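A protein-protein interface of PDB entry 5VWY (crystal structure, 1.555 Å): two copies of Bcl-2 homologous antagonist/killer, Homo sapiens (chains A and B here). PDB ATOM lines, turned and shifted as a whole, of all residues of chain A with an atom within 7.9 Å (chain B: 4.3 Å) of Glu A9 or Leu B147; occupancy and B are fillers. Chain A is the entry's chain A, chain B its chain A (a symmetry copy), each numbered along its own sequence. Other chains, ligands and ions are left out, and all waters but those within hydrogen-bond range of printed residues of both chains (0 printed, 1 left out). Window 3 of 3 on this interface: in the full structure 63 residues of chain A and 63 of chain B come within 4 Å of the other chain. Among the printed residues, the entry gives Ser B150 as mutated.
The backbone carbonyl oxygen (O) of Val A11 sits at hydrogen-bond distance from the side-chain hydroxyl (OG1) of Thr A15, at 2.7 Å.
Among the printed residues, merely in contact across the chains: Thr A15 with Met B146 (3.2 Å), Ala A12 with Val B143 (3.6 Å), Glu A9 with Leu B147 (3.9 Å) and Glu A8 with Leu B147 (3.9 Å).
Printed residues of chain B within 4 Å of Glu A9: Leu B147. Of chain A, only Glu A8 (3.9 Å) and Glu A9 (3.9 Å) come within 4 Å of Leu B147. Of the printed residues of chain B, Thr A15 touches Met B146. Printed residues of chain A within 4 Å of Met B146: Thr A15. Of the printed residues of chain A, Val B143 touches Ala A12 (3.6 Å). Printed residues of chain B within 4 Å of Glu A8: Leu B147. Val A11 touches none of the printed residues of chain B. Ser A7 touches none of the printed residues of chain B. The nearest printed residue of chain B that does not touch Thr A15 is Val B143 (4.2 Å).
Printed residues of chain A that touch a printed residue of chain B: Glu A8, Glu A9, Ala A12 and Thr A15. Among the printed residues, 4 pairs touch across the chains. Among the printed residues, no Asp or Glu carboxylate lies within 4 Å of a Lys or Arg side-chain nitrogen of the other chain.
No position is printed for both chains. Of the 4 pairs that touch across the chains among the printed residues, none has its exchanged pair printed and touching as well.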
ATOM      1  N   SER A   7      10.271  -1.789   0.047  1.00  0.00           N
ATOM      2  CA  SER A   7      11.620  -1.650   0.582  1.00  0.00           C
ATOM      3  C   SER A   7      12.614  -2.426  -0.279  1.00  0.00           C
ATOM      4  O   SER A   7      12.223  -3.222  -1.137  1.00  0.00           O
ATOM      5  CB  SER A   7      11.678  -2.135   2.032  1.00  0.00           C
ATOM      6  OG  SER A   7      11.545  -3.546   2.109  1.00  0.00           O
ATOM      7  N   GLU A   8      13.911  -2.201  -0.064  1.00  0.00           N
ATOM      8  CA  GLU A   8      14.881  -2.966  -0.833  1.00  0.00           C
ATOM      9  C   GLU A   8      15.117  -4.350  -0.239  1.00  0.00           C
ATOM     10  O   GLU A   8      15.623  -5.232  -0.942  1.00  0.00           O
ATOM     11  CB  GLU A   8      16.190  -2.177  -0.986  1.00  0.00           C
ATOM     12  CG  GLU A   8      16.876  -1.747   0.284  1.00  0.00           C
ATOM     13  CD  GLU A   8      17.805  -0.558   0.060  1.00  0.00           C
ATOM     14  OE1 GLU A   8      17.302   0.579  -0.062  1.00  0.00           O
ATOM     15  OE2 GLU A   8      19.037  -0.753   0.002  1.00  0.00           O
ATOM     16  N   GLU A   9      14.728  -4.571   1.023  1.00  0.00           N
ATOM     17  CA  GLU A   9      14.658  -5.935   1.543  1.00  0.00           C
ATOM     18  C   GLU A   9      13.611  -6.750   0.793  1.00  0.00           C
ATOM     19  O   GLU A   9      13.824  -7.933   0.502  1.00  0.00           O
ATOM     20  CB  GLU A   9      14.350  -5.921   3.042  1.00  0.00           C
ATOM     21  CG  GLU A   9      15.548  -5.648   3.949  1.00  0.00           C
ATOM     22  CD  GLU A   9      16.421  -6.873   4.148  1.00  0.00           C
ATOM     23  OE1 GLU A   9      16.122  -7.921   3.536  1.00  0.00           O
ATOM     24  OE2 GLU A   9      17.401  -6.793   4.921  1.00  0.00           O
ATOM     25  N   GLN A  10      12.460  -6.136   0.490  1.00  0.00           N
ATOM     26  CA  GLN A  10      11.461  -6.790  -0.352  1.00  0.00           C
ATOM     27  C   GLN A  10      12.012  -7.083  -1.743  1.00  0.00           C
ATOM     28  O   GLN A  10      11.863  -8.195  -2.265  1.00  0.00           O
ATOM     29  CB  GLN A  10      10.207  -5.919  -0.448  1.00  0.00           C
ATOM     30  CG  GLN A  10       9.254  -6.328  -1.560  1.00  0.00           C
ATOM     31  CD  GLN A  10       7.885  -5.687  -1.421  1.00  0.00           C
ATOM     32  OE1 GLN A  10       7.568  -5.087  -0.395  1.00  0.00           O
ATOM     33  NE2 GLN A  10       7.066  -5.815  -2.457  1.00  0.00           N
ATOM     34  N   VAL A  11      12.646  -6.088  -2.369  1.00  0.00           N
ATOM     35  CA  VAL A  11      13.209  -6.297  -3.698  1.00  0.00           C
ATOM     36  C   VAL A  11      14.244  -7.411  -3.662  1.00  0.00           C
ATOM     37  O   VAL A  11      14.281  -8.268  -4.550  1.00  0.00           O
ATOM     38  CB  VAL A  11      13.808  -4.989  -4.247  1.00  0.00           C
ATOM     39  CG1 VAL A  11      14.517  -5.249  -5.562  1.00  0.00           C
ATOM     40  CG2 VAL A  11      12.712  -3.935  -4.418  1.00  0.00           C
ATOM     41  N   ALA A  12      15.068  -7.443  -2.607  1.00  0.00           N
ATOM     42  CA  ALA A  12      16.046  -8.521  -2.453  1.00  0.00           C
ATOM     43  C   ALA A  12      15.370  -9.884  -2.343  1.00  0.00           C
ATOM     44  O   ALA A  12      15.820 -10.855  -2.963  1.00  0.00           O
ATOM     45  CB  ALA A  12      16.922  -8.266  -1.224  1.00  0.00           C
ATOM     46  N   GLN A  13      14.291  -9.980  -1.559  1.00  0.00           N
ATOM     47  CA  GLN A  13      13.552 -11.241  -1.464  1.00  0.00           C
ATOM     48  C   GLN A  13      12.991 -11.659  -2.819  1.00  0.00           C
ATOM     49  O   GLN A  13      13.131 -12.819  -3.229  1.00  0.00           O
ATOM     50  CB  GLN A  13      12.427 -11.114  -0.428  1.00  0.00           C
ATOM     51  CG  GLN A  13      11.310 -12.168  -0.536  1.00  0.00           C
ATOM     52  CD  GLN A  13      11.758 -13.572  -0.144  1.00  0.00           C
ATOM     53  OE1 GLN A  13      12.781 -13.751   0.517  1.00  0.00           O
ATOM     54  NE2 GLN A  13      10.984 -14.576  -0.552  1.00  0.00           N
ATOM     55  N   ASP A  14      12.372 -10.722  -3.541  1.00  0.00           N
ATOM     56  CA  ASP A  14      11.850 -11.020  -4.870  1.00  0.00           C
ATOM     57  C   ASP A  14      12.941 -11.479  -5.825  1.00  0.00           C
ATOM     58  O   ASP A  14      12.674 -12.253  -6.755  1.00  0.00           O
ATOM     59  CB  ASP A  14      11.163  -9.781  -5.450  1.00  0.00           C
ATOM     60  CG  ASP A  14       9.893  -9.421  -4.723  1.00  0.00           C
ATOM     61  OD1 ASP A  14       9.312 -10.302  -4.038  1.00  0.00           O
ATOM     62  OD2 ASP A  14       9.479  -8.241  -4.836  1.00  0.00           O
ATOM     63  N   THR A  15      14.169 -11.000  -5.626  1.00  0.00           N
ATOM     64  CA  THR A  15      15.254 -11.345  -6.527  1.00  0.00           C
ATOM     65  C   THR A  15      15.504 -12.845  -6.565  1.00  0.00           C
ATOM     66  O   THR A  15      15.838 -13.380  -7.624  1.00  0.00           O
ATOM     67  CB  THR A  15      16.517 -10.590  -6.117  1.00  0.00           C
ATOM     68  OG1 THR A  15      16.225  -9.196  -6.109  1.00  0.00           O
ATOM     69  CG2 THR A  15      17.660 -10.864  -7.082  1.00  0.00           C
ATOM     70  N   VAL B 143      21.532 -11.977  -4.599  1.00  0.00           N
ATOM     71  CA  VAL B 143      20.682 -11.269  -3.649  1.00  0.00           C
ATOM     72  C   VAL B 143      21.523 -10.382  -2.748  1.00  0.00           C
ATOM     73  O   VAL B 143      21.220  -9.199  -2.543  1.00  0.00           O
ATOM     74  CB  VAL B 143      19.854 -12.267  -2.825  1.00  0.00           C
ATOM     75  CG1 VAL B 143      19.106 -11.536  -1.706  1.00  0.00           C
ATOM     76  CG2 VAL B 143      18.904 -13.038  -3.739  1.00  0.00           C
ATOM     77  N   ASP B 144      22.612 -10.938  -2.220  1.00  0.00           N
ATOM     78  CA  ASP B 144      23.458 -10.190  -1.304  1.00  0.00           C
ATOM     79  C   ASP B 144      24.035  -8.959  -1.985  1.00  0.00           C
ATOM     80  O   ASP B 144      24.042  -7.865  -1.405  1.00  0.00           O
ATOM     81  CB  ASP B 144      24.570 -11.095  -0.770  1.00  0.00           C
ATOM     82  CG  ASP B 144      25.375 -10.438   0.317  1.00  0.00           C
ATOM     83  OD1 ASP B 144      24.975 -10.543   1.494  1.00  0.00           O
ATOM     84  OD2 ASP B 144      26.404  -9.812  -0.010  1.00  0.00           O
ATOM     85  N   PHE B 145      24.499  -9.109  -3.228  1.00  0.00           N
ATOM     86  CA  PHE B 145      25.046  -7.961  -3.942  1.00  0.00           C
ATOM     87  C   PHE B 145      23.978  -6.903  -4.175  1.00  0.00           C
ATOM     88  O   PHE B 145      24.210  -5.707  -3.955  1.00  0.00           O
ATOM     89  CB  PHE B 145      25.662  -8.389  -5.279  1.00  0.00           C
ATOM     90  CG  PHE B 145      26.331  -7.252  -6.003  1.00  0.00           C
ATOM     91  CD1 PHE B 145      27.642  -6.915  -5.721  1.00  0.00           C
ATOM     92  CD2 PHE B 145      25.631  -6.479  -6.928  1.00  0.00           C
ATOM     93  CE1 PHE B 145      28.264  -5.841  -6.346  1.00  0.00           C
ATOM     94  CE2 PHE B 145      26.241  -5.412  -7.560  1.00  0.00           C
ATOM     95  CZ  PHE B 145      27.558  -5.088  -7.279  1.00  0.00           C
ATOM     96  N   MET B 146      22.787  -7.318  -4.604  1.00  0.00           N
ATOM     97  CA  MET B 146      21.742  -6.340  -4.877  1.00  0.00           C
ATOM     98  C   MET B 146      21.362  -5.575  -3.619  1.00  0.00           C
ATOM     99  O   MET B 146      21.128  -4.360  -3.664  1.00  0.00           O
ATOM    100  CB  MET B 146      20.530  -7.034  -5.474  1.00  0.00           C
ATOM    101  CG  MET B 146      20.878  -7.695  -6.778  1.00  0.00           C
ATOM    102  SD  MET B 146      19.580  -7.537  -7.973  1.00  0.00           S
ATOM    103  CE  MET B 146      18.241  -6.881  -6.977  1.00  0.00           C
ATOM    104  N   LEU B 147      21.308  -6.268  -2.483  1.00  0.00           N
ATOM    105  CA  LEU B 147      20.938  -5.623  -1.232  1.00  0.00           C
ATOM    106  C   LEU B 147      22.028  -4.677  -0.734  1.00  0.00           C
ATOM    107  O   LEU B 147      21.726  -3.573  -0.263  1.00  0.00           O
ATOM    108  CB  LEU B 147      20.642  -6.691  -0.178  1.00  0.00           C
ATOM    109  CG  LEU B 147      20.220  -6.184   1.195  1.00  0.00           C
ATOM    110  CD1 LEU B 147      18.926  -5.406   1.085  1.00  0.00           C
ATOM    111  CD2 LEU B 147      20.067  -7.345   2.163  1.00  0.00           C
ATOM    112  N   HIS B 148      23.294  -5.093  -0.793  1.00  0.00           N
ATOM    113  CA  HIS B 148      24.358  -4.362  -0.110  1.00  0.00           C
ATOM    114  C   HIS B 148      25.134  -3.439  -1.028  1.00  0.00           C
ATOM    115  O   HIS B 148      26.027  -2.725  -0.557  1.00  0.00           O
ATOM    116  CB  HIS B 148      25.331  -5.333   0.566  1.00  0.00           C
ATOM    117  CG  HIS B 148      24.719  -6.111   1.689  1.00  0.00           C
ATOM    118  ND1 HIS B 148      24.498  -5.570   2.937  1.00  0.00           N
ATOM    119  CD2 HIS B 148      24.281  -7.392   1.752  1.00  0.00           C
ATOM    120  CE1 HIS B 148      23.947  -6.483   3.719  1.00  0.00           C
ATOM    121  NE2 HIS B 148      23.803  -7.596   3.022  1.00  0.00           N
ATOM    122  N   HIS B 149      24.832  -3.448  -2.321  1.00  0.00           N
ATOM    123  CA  HIS B 149      25.500  -2.590  -3.286  1.00  0.00           C
ATOM    124  C   HIS B 149      24.497  -1.740  -4.044  1.00  0.00           C
ATOM    125  O   HIS B 149      24.776  -1.312  -5.173  1.00  0.00           O
ATOM    126  CB  HIS B 149      26.366  -3.427  -4.228  1.00  0.00           C
ATOM    127  CG  HIS B 149      27.505  -4.096  -3.523  1.00  0.00           C
ATOM    128  ND1 HIS B 149      28.785  -3.584  -3.524  1.00  0.00           N
ATOM    129  CD2 HIS B 149      27.545  -5.208  -2.750  1.00  0.00           C
ATOM    130  CE1 HIS B 149      29.570  -4.366  -2.802  1.00  0.00           C
ATOM    131  NE2 HIS B 149      28.842  -5.357  -2.319  1.00  0.00           N
ATOM    132  N   SER B 150      23.316  -1.535  -3.449  1.00  0.00           N
ATOM    133  CA  SER B 150      22.323  -0.536  -3.829  1.00  0.00           C
ATOM    134  C   SER B 150      21.563  -0.860  -5.107  1.00  0.00           C
ATOM    135  O   SER B 150      20.844   0.003  -5.616  1.00  0.00           O
ATOM    136  CB  SER B 150      22.953   0.854  -3.946  1.00  0.00           C
ATOM    137  OG  SER B 150      23.566   1.196  -2.718  1.00  0.00           O
